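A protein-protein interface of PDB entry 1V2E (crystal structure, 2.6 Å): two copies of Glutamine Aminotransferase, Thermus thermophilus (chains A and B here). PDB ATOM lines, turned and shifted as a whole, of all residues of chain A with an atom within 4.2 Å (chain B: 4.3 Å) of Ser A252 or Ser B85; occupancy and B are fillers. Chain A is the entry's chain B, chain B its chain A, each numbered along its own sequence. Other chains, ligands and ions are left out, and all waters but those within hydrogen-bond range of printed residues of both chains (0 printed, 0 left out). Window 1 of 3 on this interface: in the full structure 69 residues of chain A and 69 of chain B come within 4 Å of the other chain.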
ATOM      1  N   SER A  85      22.173 -11.742  -2.970  1.00  0.00           N
ATOM      2  CA  SER A  85      22.851 -12.992  -3.304  1.00  0.00           C
ATOM      3  C   SER A  85      21.820 -13.981  -3.846  1.00  0.00           C
ATOM      4  O   SER A  85      21.526 -15.000  -3.222  1.00  0.00           O
ATOM      5  CB  SER A  85      23.506 -13.581  -2.061  1.00  0.00           C
ATOM      6  OG  SER A  85      24.504 -12.715  -1.553  1.00  0.00           O
ATOM      7  N   GLU A  89      17.770 -14.877  -1.603  1.00  0.00           N
ATOM      8  CA  GLU A  89      18.096 -13.987  -0.501  1.00  0.00           C
ATOM      9  C   GLU A  89      17.152 -12.810  -0.508  1.00  0.00           C
ATOM     10  O   GLU A  89      16.930 -12.191   0.529  1.00  0.00           O
ATOM     11  CB  GLU A  89      19.540 -13.492  -0.557  1.00  0.00           C
ATOM     12  CG  GLU A  89      19.938 -12.810   0.734  1.00  0.00           C
ATOM     13  CD  GLU A  89      21.350 -12.274   0.740  1.00  0.00           C
ATOM     14  OE1 GLU A  89      21.720 -11.546  -0.202  1.00  0.00           O
ATOM     15  OE2 GLU A  89      22.087 -12.571   1.700  1.00  0.00           O
ATOM     16  N   ARG A 248      20.209  -7.630   4.482  1.00  0.00           N
ATOM     17  CA  ARG A 248      21.081  -8.513   3.695  1.00  0.00           C
ATOM     18  C   ARG A 248      22.551  -8.246   4.011  1.00  0.00           C
ATOM     19  O   ARG A 248      23.421  -9.062   3.732  1.00  0.00           O
ATOM     20  CB  ARG A 248      20.829  -8.321   2.194  1.00  0.00           C
ATOM     21  CG  ARG A 248      21.181  -6.941   1.645  1.00  0.00           C
ATOM     22  CD  ARG A 248      22.627  -6.854   1.160  1.00  0.00           C
ATOM     23  NE  ARG A 248      22.837  -7.608  -0.077  1.00  0.00           N
ATOM     24  CZ  ARG A 248      23.567  -8.717  -0.163  1.00  0.00           C
ATOM     25  NH1 ARG A 248      24.160  -9.200   0.915  1.00  0.00           N
ATOM     26  NH2 ARG A 248      23.702  -9.345  -1.318  1.00  0.00           N
ATOM     27  N   TRP A 250      23.784  -8.132   6.904  1.00  0.00           N
ATOM     28  CA  TRP A 250      24.077  -9.091   7.967  1.00  0.00           C
ATOM     29  C   TRP A 250      24.012 -10.549   7.542  1.00  0.00           C
ATOM     30  O   TRP A 250      24.561 -11.413   8.225  1.00  0.00           O
ATOM     31  CB  TRP A 250      23.114  -8.890   9.133  1.00  0.00           C
ATOM     32  CG  TRP A 250      23.037  -7.494   9.645  1.00  0.00           C
ATOM     33  CD1 TRP A 250      21.901  -6.771   9.886  1.00  0.00           C
ATOM     34  CD2 TRP A 250      24.131  -6.664  10.037  1.00  0.00           C
ATOM     35  NE1 TRP A 250      22.223  -5.543  10.406  1.00  0.00           N
ATOM     36  CE2 TRP A 250      23.587  -5.451  10.509  1.00  0.00           C
ATOM     37  CE3 TRP A 250      25.518  -6.824  10.039  1.00  0.00           C
ATOM     38  CZ2 TRP A 250      24.388  -4.406  10.977  1.00  0.00           C
ATOM     39  CZ3 TRP A 250      26.315  -5.778  10.508  1.00  0.00           C
ATOM     40  CH2 TRP A 250      25.746  -4.590  10.967  1.00  0.00           C
ATOM     41  N   THR A 251      23.325 -10.834   6.442  1.00  0.00           N
ATOM     42  CA  THR A 251      23.230 -12.206   5.971  1.00  0.00           C
ATOM     43  C   THR A 251      24.468 -12.601   5.169  1.00  0.00           C
ATOM     44  O   THR A 251      25.248 -13.426   5.628  1.00  0.00           O
ATOM     45  CB  THR A 251      21.960 -12.432   5.126  1.00  0.00           C
ATOM     46  OG1 THR A 251      21.930 -11.514   4.034  1.00  0.00           O
ATOM     47  CG2 THR A 251      20.718 -12.249   5.990  1.00  0.00           C
ATOM     48  N   SER A 252      24.670 -12.011   3.994  1.00  0.00           N
ATOM     49  CA  SER A 252      25.849 -12.328   3.178  1.00  0.00           C
ATOM     50  C   SER A 252      26.640 -11.074   2.750  1.00  0.00           C
ATOM     51  O   SER A 252      27.367 -11.096   1.760  1.00  0.00           O
ATOM     52  CB  SER A 252      25.418 -13.110   1.933  1.00  0.00           C
ATOM     53  OG  SER A 252      24.652 -12.314   1.038  1.00  0.00           O
ATOM     54  N   PHE A 253      26.498  -9.994   3.516  1.00  0.00           N
ATOM     55  CA  PHE A 253      27.143  -8.711   3.247  1.00  0.00           C
ATOM     56  C   PHE A 253      26.847  -8.098   1.873  1.00  0.00           C
ATOM     57  O   PHE A 253      26.273  -7.021   1.798  1.00  0.00           O
ATOM     58  CB  PHE A 253      28.646  -8.778   3.436  1.00  0.00           C
ATOM     59  CG  PHE A 253      29.275  -7.423   3.483  1.00  0.00           C
ATOM     60  CD1 PHE A 253      29.138  -6.623   4.619  1.00  0.00           C
ATOM     61  CD2 PHE A 253      29.911  -6.896   2.363  1.00  0.00           C
ATOM     62  CE1 PHE A 253      29.619  -5.312   4.636  1.00  0.00           C
ATOM     63  CE2 PHE A 253      30.394  -5.586   2.371  1.00  0.00           C
ATOM     64  CZ  PHE A 253      30.246  -4.793   3.512  1.00  0.00           C
ATOM     65  N   SER A 254      27.274  -8.747   0.794  1.00  0.00           N
ATOM     66  CA  SER A 254      26.980  -8.264  -0.553  1.00  0.00           C
ATOM     67  C   SER A 254      27.208  -9.377  -1.519  1.00  0.00           C
ATOM     68  O   SER A 254      27.791 -10.384  -1.166  1.00  0.00           O
ATOM     69  CB  SER A 254      27.823  -7.046  -0.955  1.00  0.00           C
ATOM     70  OG  SER A 254      29.183  -7.173  -0.598  1.00  0.00           O
ATOM     71  N   THR B  84      29.379 -21.727   2.893  1.00  0.00           N
ATOM     72  CA  THR B  84      28.437 -20.622   2.966  1.00  0.00           C
ATOM     73  C   THR B  84      28.837 -19.488   2.029  1.00  0.00           C
ATOM     74  O   THR B  84      29.941 -19.473   1.476  1.00  0.00           O
ATOM     75  CB  THR B  84      28.396 -20.054   4.392  1.00  0.00           C
ATOM     76  OG1 THR B  84      29.694 -19.560   4.727  1.00  0.00           O
ATOM     77  CG2 THR B  84      28.013 -21.131   5.400  1.00  0.00           C
ATOM     78  N   SER B  85      27.926 -18.537   1.861  1.00  0.00           N
ATOM     79  CA  SER B  85      28.175 -17.374   1.029  1.00  0.00           C
ATOM     80  C   SER B  85      28.960 -16.367   1.861  1.00  0.00           C
ATOM     81  O   SER B  85      28.476 -15.278   2.147  1.00  0.00           O
ATOM     82  CB  SER B  85      26.859 -16.764   0.577  1.00  0.00           C
ATOM     83  OG  SER B  85      26.129 -17.696  -0.204  1.00  0.00           O
ATOM     84  N   GLY B  86      30.176 -16.748   2.244  1.00  0.00           N
ATOM     85  CA  GLY B  86      31.015 -15.885   3.050  1.00  0.00           C
ATOM     86  C   GLY B  86      30.975 -16.241   4.529  1.00  0.00           C
ATOM     87  O   GLY B  86      30.060 -16.912   5.013  1.00  0.00           O
ATOM     88  N   THR B  88      30.383 -14.253   6.611  1.00  0.00           N
ATOM     89  CA  THR B  88      29.282 -13.416   7.084  1.00  0.00           C
ATOM     90  C   THR B  88      28.005 -14.232   7.240  1.00  0.00           C
ATOM     91  O   THR B  88      27.293 -14.107   8.244  1.00  0.00           O
ATOM     92  CB  THR B  88      29.009 -12.231   6.106  1.00  0.00           C
ATOM     93  OG1 THR B  88      30.106 -11.313   6.144  1.00  0.00           O
ATOM     94  CG2 THR B  88      27.755 -11.483   6.494  1.00  0.00           C
ATOM     95  N   GLU B  89      27.721 -15.063   6.242  1.00  0.00           N
ATOM     96  CA  GLU B  89      26.532 -15.901   6.262  1.00  0.00           C
ATOM     97  C   GLU B  89      26.708 -17.087   7.200  1.00  0.00           C
ATOM     98  O   GLU B  89      25.732 -17.700   7.626  1.00  0.00           O
ATOM     99  CB  GLU B  89      26.228 -16.421   4.868  1.00  0.00           C
ATOM    100  CG  GLU B  89      24.908 -17.139   4.787  1.00  0.00           C
ATOM    101  CD  GLU B  89      24.774 -17.928   3.520  1.00  0.00           C
ATOM    102  OE1 GLU B  89      25.639 -18.790   3.277  1.00  0.00           O
ATOM    103  OE2 GLU B  89      23.814 -17.699   2.763  1.00  0.00           O
ATOM    104  N   ARG B 230      32.726 -14.126  -1.842  1.00  0.00           N
ATOM    105  CA  ARG B 230      31.642 -14.643  -0.989  1.00  0.00           C
ATOM    106  C   ARG B 230      31.587 -16.175  -0.879  1.00  0.00           C
ATOM    107  O   ARG B 230      30.561 -16.797  -1.164  1.00  0.00           O
ATOM    108  CB  ARG B 230      30.276 -14.138  -1.490  1.00  0.00           C
ATOM    109  CG  ARG B 230      30.256 -12.686  -1.948  1.00  0.00           C
ATOM    110  CD  ARG B 230      30.948 -11.786  -0.958  1.00  0.00           C
ATOM    111  NE  ARG B 230      30.338 -11.885   0.358  1.00  0.00           N
ATOM    112  CZ  ARG B 230      31.011 -11.783   1.494  1.00  0.00           C
ATOM    113  NH1 ARG B 230      32.319 -11.585   1.464  1.00  0.00           N
ATOM    114  NH2 ARG B 230      30.378 -11.874   2.658  1.00  0.00           N
ATOM    115  N   ARG B 248      21.369 -22.143   5.876  1.00  0.00           N
ATOM    116  CA  ARG B 248      21.974 -21.319   4.828  1.00  0.00           C
ATOM    117  C   ARG B 248      21.295 -21.490   3.481  1.00  0.00           C
ATOM    118  O   ARG B 248      21.360 -20.603   2.626  1.00  0.00           O
ATOM    119  CB  ARG B 248      23.492 -21.602   4.711  1.00  0.00           C
ATOM    120  CG  ARG B 248      23.908 -22.940   4.083  1.00  0.00           C
ATOM    121  CD  ARG B 248      23.799 -22.953   2.547  1.00  0.00           C
ATOM    122  NE  ARG B 248      24.955 -22.386   1.838  1.00  0.00           N
ATOM    123  CZ  ARG B 248      25.102 -21.111   1.474  1.00  0.00           C
ATOM    124  NH1 ARG B 248      24.167 -20.213   1.739  1.00  0.00           N
ATOM    125  NH2 ARG B 248      26.195 -20.734   0.826  1.00  0.00           N
ATOM    126  N   SER B 252      20.471 -18.003   1.199  1.00  0.00           N
ATOM    127  CA  SER B 252      20.899 -17.734  -0.174  1.00  0.00           C
ATOM    128  C   SER B 252      21.055 -18.976  -1.047  1.00  0.00           C
ATOM    129  O   SER B 252      21.365 -18.854  -2.231  1.00  0.00           O
ATOM    130  CB  SER B 252      22.191 -16.911  -0.195  1.00  0.00           C
ATOM    131  OG  SER B 252      23.261 -17.603   0.407  1.00  0.00           O
ATOM    132  N   SER B 254      23.175 -21.560  -2.046  1.00  0.00           N
ATOM    133  CA  SER B 254      24.567 -22.009  -2.104  1.00  0.00           C
ATOM    134  C   SER B 254      25.444 -20.908  -2.707  1.00  0.00           C
ATOM    135  O   SER B 254      24.943 -20.002  -3.368  1.00  0.00           O
ATOM    136  CB  SER B 254      24.704 -23.296  -2.916  1.00  0.00           C
ATOM    137  OG  SER B 254      24.335 -23.083  -4.260  1.00  0.00           O
ATOM    138  N   ALA B 255      26.748 -21.004  -2.477  1.00  0.00           N
ATOM    139  CA  ALA B 255      27.712 -20.028  -2.946  1.00  0.00           C
ATOM    140  C   ALA B 255      27.905 -20.085  -4.441  1.00  0.00           C
ATOM    141  O   ALA B 255      27.514 -21.059  -5.066  1.00  0.00           O
ATOM    142  CB  ALA B 255      29.024 -20.252  -2.251  1.00  0.00           C
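The backbone carbonyl oxygen of Thr B88 lies close to the backbone carbonyl oxygen of Thr A251 (3.4 Å).
The backbone NH (N) of Glu B89 sits close to the backbone carbonyl oxygen (O) of Thr A251, 3.0 Å away.
NE of Arg B230 lies within hydrogen-bond range of O of Ser A254, 3.3 Å away.
The guanidinium group (NH2) of Arg B230 is in hydrogen-bond range of the backbone carbonyl oxygen (O) of Ser A252, at 3.2 Å.
The backbone NH (N) of Ser B85 is in hydrogen-bond range of the side-chain carboxylate (OE1) of Glu B89 (2.7 Å).
The side-chain carboxylate (OE1) of Glu B89 is in salt-bridge range of the guanidinium group (NH1) of Arg B248.
O of Phe A253 lies close to NH1 of Arg A248 (3.2 Å).
The backbone carbonyl oxygen (O) of Arg B230 is in hydrogen-bond range of the backbone NH (N) of Gly B86 (3.4 Å).
The guanidinium group (NH1) of Arg B248 lies within hydrogen-bond range of the side-chain hydroxyl (OG) of Ser B252 (3.1 Å).
The side-chain hydroxyl (OG) of Ser B252 is in hydrogen-bond range of the side-chain carboxylate (OE2) of Glu B89.
Among the printed residues, pairs that only touch across the chains: Ser A85 with Ser B252 (3.6 Å), Trp A250 with Thr B88 (3.6 Å), Ser A252 with Ser B85 (3.8 Å), Ser A252 with Thr B88 (3.9 Å), Phe A253 with Thr B88 (3.6 Å) and Phe A253 with Arg B230 (3.6 Å).
Ser A252 touches just these residues of chain B: Ser B85 (3.8 Å), Thr B88 (3.9 Å) and Arg B230 (3.2 Å).
Of the printed residues of chain A, Ser B85 touches Ser A252 (3.8 Å).
Of the printed residues of chain A, Ser B252 touches Ser A85 (3.6 Å).
Printed residues of chain B within 4 Å of Trp A250: Thr B88.
Ser B254 touches none of the printed residues of chain A.
Arg B248 touches none of the printed residues of chain A.
The nearest printed residue of chain B that does not touch Ser A252 is Glu B89 (4.4 Å).
Hydrophobic or aromatic side chains of chain A within 4 Å of the printed part of chain B: Phe A253.
Among the printed residues, no Asp or Glu carboxylate lies within 4 Å of a Lys or Arg side-chain nitrogen of the other chain.
Ser A85 touches Ser B252, and with the chains exchanged Ser A252 touches Ser B85.
Positions printed for both chains: 85, 89, 248, 252 and 254.
Of the 10 pairs that touch across the chains among the printed residues, 2 have their exchanged pair printed and touching as well.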
